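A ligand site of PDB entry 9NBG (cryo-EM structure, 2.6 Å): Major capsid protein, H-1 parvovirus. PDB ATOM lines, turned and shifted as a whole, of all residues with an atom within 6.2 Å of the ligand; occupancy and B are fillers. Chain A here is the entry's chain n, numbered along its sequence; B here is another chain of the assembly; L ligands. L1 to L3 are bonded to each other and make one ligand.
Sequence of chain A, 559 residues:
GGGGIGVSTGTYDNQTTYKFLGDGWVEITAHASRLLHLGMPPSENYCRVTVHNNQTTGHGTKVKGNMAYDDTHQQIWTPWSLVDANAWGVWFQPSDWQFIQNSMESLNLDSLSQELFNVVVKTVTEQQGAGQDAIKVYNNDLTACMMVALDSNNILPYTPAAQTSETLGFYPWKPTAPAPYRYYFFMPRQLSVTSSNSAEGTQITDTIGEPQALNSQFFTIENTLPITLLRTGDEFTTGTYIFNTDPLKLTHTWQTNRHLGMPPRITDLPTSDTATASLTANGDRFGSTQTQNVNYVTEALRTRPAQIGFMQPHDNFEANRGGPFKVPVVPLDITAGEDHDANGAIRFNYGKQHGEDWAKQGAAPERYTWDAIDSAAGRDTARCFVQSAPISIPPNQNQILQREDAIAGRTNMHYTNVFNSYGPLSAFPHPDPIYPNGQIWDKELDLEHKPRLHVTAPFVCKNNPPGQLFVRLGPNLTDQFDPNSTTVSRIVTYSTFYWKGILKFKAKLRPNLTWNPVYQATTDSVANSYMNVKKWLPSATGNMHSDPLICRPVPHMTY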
ATOM      1  N   HIS A 340       4.231 -11.932   6.456  1.00  0.00           N
ATOM      2  CA  HIS A 340       4.559 -11.686   7.877  1.00  0.00           C
ATOM      3  C   HIS A 340       5.089 -12.960   8.553  1.00  0.00           C
ATOM      4  O   HIS A 340       6.164 -12.893   9.190  1.00  0.00           O
ATOM      5  CB  HIS A 340       3.353 -11.098   8.614  1.00  0.00           C
ATOM      6  CG  HIS A 340       2.981  -9.724   8.143  1.00  0.00           C
ATOM      7  ND1 HIS A 340       2.602  -8.717   9.008  1.00  0.00           N
ATOM      8  CD2 HIS A 340       2.928  -9.191   6.912  1.00  0.00           C
ATOM      9  CE1 HIS A 340       2.329  -7.631   8.311  1.00  0.00           C
ATOM     10  NE2 HIS A 340       2.512  -7.895   7.038  1.00  0.00           N
ATOM     11  N   ARG A 347       2.987  -9.655  16.407  1.00  0.00           N
ATOM     12  CA  ARG A 347       1.699  -8.972  16.708  1.00  0.00           C
ATOM     13  C   ARG A 347       1.478  -9.023  18.220  1.00  0.00           C
ATOM     14  O   ARG A 347       1.442 -10.131  18.766  1.00  0.00           O
ATOM     15  CB  ARG A 347       0.544  -9.642  15.959  1.00  0.00           C
ATOM     16  CG  ARG A 347      -0.795  -8.948  16.135  1.00  0.00           C
ATOM     17  CD  ARG A 347      -1.832  -9.470  15.167  1.00  0.00           C
ATOM     18  NE  ARG A 347      -3.118  -8.783  15.212  1.00  0.00           N
ATOM     19  CZ  ARG A 347      -3.316  -7.515  14.881  1.00  0.00           C
ATOM     20  NH1 ARG A 347      -2.297  -6.718  14.618  1.00  0.00           N
ATOM     21  NH2 ARG A 347      -4.550  -7.047  14.797  1.00  0.00           N
ATOM     22  N   TYR A 350      -2.204  -5.267  23.846  1.00  0.00           N
ATOM     23  CA  TYR A 350      -1.891  -4.534  25.099  1.00  0.00           C
ATOM     24  C   TYR A 350      -3.126  -3.812  25.639  1.00  0.00           C
ATOM     25  O   TYR A 350      -4.160  -3.798  24.936  1.00  0.00           O
ATOM     26  CB  TYR A 350      -0.733  -3.557  24.889  1.00  0.00           C
ATOM     27  CG  TYR A 350      -0.776  -2.714  23.638  1.00  0.00           C
ATOM     28  CD1 TYR A 350      -0.966  -1.350  23.702  1.00  0.00           C
ATOM     29  CD2 TYR A 350      -0.580  -3.286  22.385  1.00  0.00           C
ATOM     30  CE1 TYR A 350      -0.994  -0.566  22.562  1.00  0.00           C
ATOM     31  CE2 TYR A 350      -0.602  -2.508  21.234  1.00  0.00           C
ATOM     32  CZ  TYR A 350      -0.804  -1.153  21.323  1.00  0.00           C
ATOM     33  OH  TYR A 350      -0.826  -0.384  20.178  1.00  0.00           O
ATOM     34  N   GLY A 355      -0.649   1.775  26.290  1.00  0.00           N
ATOM     35  CA  GLY A 355      -0.784   2.545  25.033  1.00  0.00           C
ATOM     36  C   GLY A 355      -2.118   2.366  24.320  1.00  0.00           C
ATOM     37  O   GLY A 355      -2.307   3.024  23.288  1.00  0.00           O
ATOM     38  N   ASP A 357      -5.695   3.291  23.362  1.00  0.00           N
ATOM     39  CA  ASP A 357      -6.446   4.570  23.481  1.00  0.00           C
ATOM     40  C   ASP A 357      -7.382   4.478  24.674  1.00  0.00           C
ATOM     41  O   ASP A 357      -8.205   3.552  24.722  1.00  0.00           O
ATOM     42  CB  ASP A 357      -7.198   4.893  22.186  1.00  0.00           C
ATOM     43  CG  ASP A 357      -7.828   6.288  22.186  1.00  0.00           C
ATOM     44  OD1 ASP A 357      -7.648   7.020  23.179  1.00  0.00           O
ATOM     45  OD2 ASP A 357      -8.487   6.617  21.184  1.00  0.00           O
ATOM     46  N   LYS A 360     -10.918   4.151  23.855  1.00  0.00           N
ATOM     47  CA  LYS A 360     -11.406   2.860  23.308  1.00  0.00           C
ATOM     48  C   LYS A 360     -12.219   2.123  24.363  1.00  0.00           C
ATOM     49  O   LYS A 360     -11.633   1.713  25.381  1.00  0.00           O
ATOM     50  CB  LYS A 360     -10.230   2.014  22.807  1.00  0.00           C
ATOM     51  CG  LYS A 360     -10.600   0.662  22.199  1.00  0.00           C
ATOM     52  CD  LYS A 360      -9.435  -0.046  21.542  1.00  0.00           C
ATOM     53  CE  LYS A 360      -9.761  -1.459  21.112  1.00  0.00           C
ATOM     54  NZ  LYS A 360      -8.585  -2.137  20.521  1.00  0.00           N
ATOM     55  N   PRO A 365      -8.618  -6.014  23.580  1.00  0.00           N
ATOM     56  CA  PRO A 365      -7.342  -5.316  23.752  1.00  0.00           C
ATOM     57  C   PRO A 365      -6.857  -4.642  22.466  1.00  0.00           C
ATOM     58  O   PRO A 365      -7.326  -5.009  21.403  1.00  0.00           O
ATOM     59  CB  PRO A 365      -6.380  -6.452  24.125  1.00  0.00           C
ATOM     60  CG  PRO A 365      -6.967  -7.661  23.442  1.00  0.00           C
ATOM     61  CD  PRO A 365      -8.464  -7.470  23.546  1.00  0.00           C
ATOM     62  N   GLU A 366      -5.896  -3.727  22.565  1.00  0.00           N
ATOM     63  CA  GLU A 366      -5.316  -3.099  21.339  1.00  0.00           C
ATOM     64  C   GLU A 366      -4.346  -4.095  20.693  1.00  0.00           C
ATOM     65  O   GLU A 366      -3.522  -4.661  21.424  1.00  0.00           O
ATOM     66  CB  GLU A 366      -4.583  -1.804  21.683  1.00  0.00           C
ATOM     67  CG  GLU A 366      -4.357  -0.914  20.480  1.00  0.00           C
ATOM     68  CD  GLU A 366      -5.635  -0.282  19.948  1.00  0.00           C
ATOM     69  OE1 GLU A 366      -6.221   0.537  20.682  1.00  0.00           O
ATOM     70  OE2 GLU A 366      -6.039  -0.633  18.825  1.00  0.00           O
ATOM     71  N   ARG A 367      -4.468  -4.319  19.384  1.00  0.00           N
ATOM     72  CA  ARG A 367      -3.607  -5.319  18.693  1.00  0.00           C
ATOM     73  C   ARG A 367      -2.773  -4.605  17.617  1.00  0.00           C
ATOM     74  O   ARG A 367      -3.376  -4.025  16.702  1.00  0.00           O
ATOM     75  CB  ARG A 367      -4.472  -6.401  18.033  1.00  0.00           C
ATOM     76  CG  ARG A 367      -5.676  -6.862  18.841  1.00  0.00           C
ATOM     77  CD  ARG A 367      -6.481  -7.888  18.070  1.00  0.00           C
ATOM     78  NE  ARG A 367      -7.720  -8.282  18.745  1.00  0.00           N
ATOM     79  CZ  ARG A 367      -7.784  -8.903  19.914  1.00  0.00           C
ATOM     80  NH1 ARG A 367      -6.721  -9.503  20.420  1.00  0.00           N
ATOM     81  NH2 ARG A 367      -8.942  -8.945  20.567  1.00  0.00           N
ATOM     82  N   TYR A 368      -1.444  -4.673  17.718  1.00  0.00           N
ATOM     83  CA  TYR A 368      -0.569  -4.050  16.695  1.00  0.00           C
ATOM     84  C   TYR A 368       0.424  -5.089  16.147  1.00  0.00           C
ATOM     85  O   TYR A 368       0.981  -5.853  16.947  1.00  0.00           O
ATOM     86  CB  TYR A 368       0.225  -2.889  17.287  1.00  0.00           C
ATOM     87  CG  TYR A 368       1.080  -2.151  16.301  1.00  0.00           C
ATOM     88  CD1 TYR A 368       0.523  -1.317  15.347  1.00  0.00           C
ATOM     89  CD2 TYR A 368       2.457  -2.307  16.291  1.00  0.00           C
ATOM     90  CE1 TYR A 368       1.295  -0.643  14.424  1.00  0.00           C
ATOM     91  CE2 TYR A 368       3.252  -1.639  15.374  1.00  0.00           C
ATOM     92  CZ  TYR A 368       2.669  -0.801  14.431  1.00  0.00           C
ATOM     93  OH  TYR A 368       3.456  -0.140  13.522  1.00  0.00           O
ATOM     94  N   THR A 369       0.629  -5.086  14.823  1.00  0.00           N
ATOM     95  CA  THR A 369       1.623  -6.011  14.209  1.00  0.00           C
ATOM     96  C   THR A 369       2.909  -5.241  13.913  1.00  0.00           C
ATOM     97  O   THR A 369       2.821  -4.207  13.233  1.00  0.00           O
ATOM     98  CB  THR A 369       1.076  -6.650  12.937  1.00  0.00           C
ATOM     99  OG1 THR A 369      -0.161  -7.287  13.247  1.00  0.00           O
ATOM    100  CG2 THR A 369       2.033  -7.662  12.323  1.00  0.00           C
ATOM    101  N   TRP A 370       4.046  -5.713  14.439  1.00  0.00           N
ATOM    102  CA  TRP A 370       5.340  -5.015  14.216  1.00  0.00           C
ATOM    103  C   TRP A 370       6.076  -5.667  13.046  1.00  0.00           C
ATOM    104  O   TRP A 370       6.442  -6.844  13.170  1.00  0.00           O
ATOM    105  CB  TRP A 370       6.202  -5.050  15.478  1.00  0.00           C
ATOM    106  CG  TRP A 370       7.513  -4.336  15.314  1.00  0.00           C
ATOM    107  CD1 TRP A 370       8.736  -4.898  15.122  1.00  0.00           C
ATOM    108  CD2 TRP A 370       7.726  -2.914  15.346  1.00  0.00           C
ATOM    109  NE1 TRP A 370       9.699  -3.930  15.024  1.00  0.00           N
ATOM    110  CE2 TRP A 370       9.109  -2.697  15.155  1.00  0.00           C
ATOM    111  CE3 TRP A 370       6.888  -1.797  15.504  1.00  0.00           C
ATOM    112  CZ2 TRP A 370       9.665  -1.424  15.119  1.00  0.00           C
ATOM    113  CZ3 TRP A 370       7.449  -0.540  15.462  1.00  0.00           C
ATOM    114  CH2 TRP A 370       8.819  -0.365  15.281  1.00  0.00           C
ATOM    115  N   ASP A 371       6.268  -4.926  11.950  1.00  0.00           N
ATOM    116  CA  ASP A 371       7.028  -5.460  10.792  1.00  0.00           C
ATOM    117  C   ASP A 371       8.472  -4.955  10.915  1.00  0.00           C
ATOM    118  O   ASP A 371       8.652  -3.759  11.214  1.00  0.00           O
ATOM    119  CB  ASP A 371       6.364  -5.072   9.472  1.00  0.00           C
ATOM    120  CG  ASP A 371       4.912  -5.530   9.388  1.00  0.00           C
ATOM    121  OD1 ASP A 371       4.465  -6.217  10.331  1.00  0.00           O
ATOM    122  OD2 ASP A 371       4.251  -5.181   8.400  1.00  0.00           O
ATOM    123  N   TYR A 530      -0.752   8.004  10.612  1.00  0.00           N
ATOM    124  CA  TYR A 530      -0.250   7.238  11.775  1.00  0.00           C
ATOM    125  C   TYR A 530       0.608   8.153  12.661  1.00  0.00           C
ATOM    126  O   TYR A 530       0.793   7.825  13.839  1.00  0.00           O
ATOM    127  CB  TYR A 530       0.580   6.038  11.319  1.00  0.00           C
ATOM    128  CG  TYR A 530       1.025   5.125  12.429  1.00  0.00           C
ATOM    129  CD1 TYR A 530       0.111   4.415  13.187  1.00  0.00           C
ATOM    130  CD2 TYR A 530       2.373   4.988  12.754  1.00  0.00           C
ATOM    131  CE1 TYR A 530       0.516   3.581  14.224  1.00  0.00           C
ATOM    132  CE2 TYR A 530       2.785   4.162  13.782  1.00  0.00           C
ATOM    133  CZ  TYR A 530       1.852   3.459  14.518  1.00  0.00           C
ATOM    134  OH  TYR A 530       2.265   2.633  15.546  1.00  0.00           O
ATOM    135  N   LYS A 535      -2.311  12.213  18.131  1.00  0.00           N
ATOM    136  CA  LYS A 535      -2.239  10.902  18.827  1.00  0.00           C
ATOM    137  C   LYS A 535      -1.413  11.005  20.106  1.00  0.00           C
ATOM    138  O   LYS A 535      -1.820  10.409  21.110  1.00  0.00           O
ATOM    139  CB  LYS A 535      -1.664   9.857  17.869  1.00  0.00           C
ATOM    140  CG  LYS A 535      -2.442   9.671  16.582  1.00  0.00           C
ATOM    141  CD  LYS A 535      -1.826   8.632  15.665  1.00  0.00           C
ATOM    142  CE  LYS A 535      -1.693   7.280  16.342  1.00  0.00           C
ATOM    143  NZ  LYS A 535      -1.064   6.287  15.439  1.00  0.00           N
ATOM    144  N   ASP A 547       0.835   4.961  20.453  1.00  0.00           N
ATOM    145  CA  ASP A 547       0.977   3.965  19.363  1.00  0.00           C
ATOM    146  C   ASP A 547       2.473   3.722  19.123  1.00  0.00           C
ATOM    147  O   ASP A 547       3.266   4.667  19.279  1.00  0.00           O
ATOM    148  CB  ASP A 547       0.249   4.417  18.099  1.00  0.00           C
ATOM    149  CG  ASP A 547      -0.880   3.480  17.693  1.00  0.00           C
ATOM    150  OD1 ASP A 547      -1.057   2.451  18.368  1.00  0.00           O
ATOM    151  OD2 ASP A 547      -1.573   3.786  16.698  1.00  0.00           O
ATOM    152  N   GLN B 292      -0.451 -13.320  12.482  1.00  0.00           N
ATOM    153  CA  GLN B 292      -1.344 -12.120  12.480  1.00  0.00           C
ATOM    154  C   GLN B 292      -2.752 -12.472  11.993  1.00  0.00           C
ATOM    155  O   GLN B 292      -3.688 -11.753  12.386  1.00  0.00           O
ATOM    156  CB  GLN B 292      -0.748 -11.034  11.580  1.00  0.00           C
ATOM    157  CG  GLN B 292      -0.483 -11.492  10.157  1.00  0.00           C
ATOM    158  CD  GLN B 292      -0.040 -10.357   9.266  1.00  0.00           C
ATOM    159  OE1 GLN B 292       0.034  -9.209   9.696  1.00  0.00           O
ATOM    160  NE2 GLN B 292       0.234 -10.668   8.017  1.00  0.00           N
ATOM    161  N   ASN B 295      -6.742 -13.023  15.790  1.00  0.00           N
ATOM    162  CA  ASN B 295      -6.836 -11.889  16.733  1.00  0.00           C
ATOM    163  C   ASN B 295      -6.978 -12.430  18.154  1.00  0.00           C
ATOM    164  O   ASN B 295      -7.790 -11.873  18.925  1.00  0.00           O
ATOM    165  CB  ASN B 295      -7.978 -10.942  16.374  1.00  0.00           C
ATOM    166  CG  ASN B 295      -7.773 -10.255  15.043  1.00  0.00           C
ATOM    167  OD1 ASN B 295      -6.766 -10.468  14.368  1.00  0.00           O
ATOM    168  ND2 ASN B 295      -8.719  -9.420  14.644  1.00  0.00           N
HETATM  169  C1  LIG L   1      -7.643  -5.066   5.598  1.00  0.00           C
HETATM  170  C2  LIG L   1      -6.313  -4.373   5.305  1.00  0.00           C
HETATM  171  C3  LIG L   1      -5.265  -4.768   6.343  1.00  0.00           C
HETATM  172  C4  LIG L   1      -5.935  -4.890   7.707  1.00  0.00           C
HETATM  173  C5  LIG L   1      -6.894  -6.083   7.693  1.00  0.00           C
HETATM  174  C6  LIG L   1      -8.017  -5.939   8.691  1.00  0.00           C
HETATM  175  C7  LIG L   1      -5.786  -3.777   2.986  1.00  0.00           C
HETATM  176  C8  LIG L   1      -6.227  -2.390   3.355  1.00  0.00           C
HETATM  177  N1  LIG L   1      -5.825  -4.682   3.965  1.00  0.00           N
HETATM  178  O1  LIG L   1      -8.510  -4.155   6.206  1.00  0.00           O
HETATM  179  O2  LIG L   1      -4.239  -3.789   6.363  1.00  0.00           O
HETATM  180  O3  LIG L   1      -4.940  -5.112   8.707  1.00  0.00           O
HETATM  181  O4  LIG L   1      -7.507  -6.247   6.394  1.00  0.00           O
HETATM  182  O5  LIG L   1      -8.874  -7.080   8.666  1.00  0.00           O
HETATM  183  O6  LIG L   1      -5.402  -4.060   1.857  1.00  0.00           O
HETATM  184  C1  LG2 L   2      -4.723  -3.952   9.544  1.00  0.00           C
HETATM  185  C2  LG2 L   2      -5.128  -4.149  10.989  1.00  0.00           C
HETATM  186  C3  LG2 L   2      -6.489  -3.550  11.282  1.00  0.00           C
HETATM  187  C4  LG2 L   2      -6.517  -2.102  10.815  1.00  0.00           C
HETATM  188  C5  LG2 L   2      -6.309  -2.101   9.318  1.00  0.00           C
HETATM  189  C6  LG2 L   2      -6.355  -0.709   8.727  1.00  0.00           C
HETATM  190  O1  LG2 L   2      -5.094  -5.540  11.321  1.00  0.00           O
HETATM  191  O2  LG2 L   2      -6.822  -3.711  12.677  1.00  0.00           O
HETATM  192  O3  LG2 L   2      -5.472  -1.344  11.403  1.00  0.00           O
HETATM  193  O4  LG2 L   2      -4.999  -2.642   9.013  1.00  0.00           O
HETATM  194  O5  LG2 L   2      -7.467   0.032   9.239  1.00  0.00           O
HETATM  195  C1  LG3 L   3      -6.461  -3.746  14.981  1.00  0.00           C
HETATM  196  C2  LG3 L   3      -6.408  -2.787  13.784  1.00  0.00           C
HETATM  197  C3  LG3 L   3      -7.108  -1.497  14.174  1.00  0.00           C
HETATM  198  C4  LG3 L   3      -6.387  -0.721  15.257  1.00  0.00           C
HETATM  199  C5  LG3 L   3      -4.904  -0.577  14.916  1.00  0.00           C
HETATM  200  C6  LG3 L   3      -4.289  -1.947  14.640  1.00  0.00           C
HETATM  201  C7  LG3 L   3      -2.851  -1.819  14.149  1.00  0.00           C
HETATM  202  C8  LG3 L   3      -2.430  -3.015  13.299  1.00  0.00           C
HETATM  203  C9  LG3 L   3      -1.021  -2.915  12.749  1.00  0.00           C
HETATM  204  C10 LG3 L   3      -4.219   1.429  16.165  1.00  0.00           C
HETATM  205  C11 LG3 L   3      -4.212   1.907  17.573  1.00  0.00           C
HETATM  206  N1  LG3 L   3      -4.192   0.099  15.993  1.00  0.00           N
HETATM  207  O1  LG3 L   3      -7.247  -3.560  15.875  1.00  0.00           O
HETATM  208  O2  LG3 L   3      -5.722  -4.705  14.993  1.00  0.00           O
HETATM  209  O3  LG3 L   3      -6.990   0.561  15.413  1.00  0.00           O
HETATM  210  O4  LG3 L   3      -5.005  -2.546  13.552  1.00  0.00           O
HETATM  211  O5  LG3 L   3      -2.702  -0.608  13.390  1.00  0.00           O
HETATM  212  O6  LG3 L   3      -2.559  -4.203  14.071  1.00  0.00           O
HETATM  213  O7  LG3 L   3      -0.692  -4.045  11.943  1.00  0.00           O
HETATM  214  O8  LG3 L   3      -4.239   2.198  15.205  1.00  0.00           O
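OD2 of Asp 547 lies close to O8 of LG3 L3 (3.4 Å). Merely in contact with the ligand: Tyr 368 (3.3 Å). Hydrophobic or aromatic side chains that line the ligand: Tyr 368.
NH2 of Arg 347 is in salt-bridge range of O2 of LG3 L3 (2.6 Å). The backbone carbonyl oxygen (O) of Arg 367 sits at hydrogen-bond distance from an oxygen (O6) of LG3 L3 (2.8 Å). OE2 of Glu 366 lies close to N1 of LG3 L3. The backbone NH (N) of Thr 369 lies close to an oxygen (O7) of LG3 L3 (3.3 Å).
OE2 of Glu 366 lies within salt-bridge range of NZ of Lys 360 (3.4 Å). NH1 of Arg 367 is in hydrogen-bond range of O of Asn 295 of chain B, at 3.0 Å. O of Glu 366 lies within hydrogen-bond range of N of Tyr 350 (2.8 Å). OD1 of Asp 547 sits at hydrogen-bond distance from OH of Tyr 350 (3.4 Å). The side-chain amino group (NZ) of Lys 535 is in salt-bridge range of the side-chain carboxylate (OD2) of Asp 547 (2.8 Å). NH1 of Arg 347 is in hydrogen-bond range of OG1 of Thr 369, 2.6 Å away.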
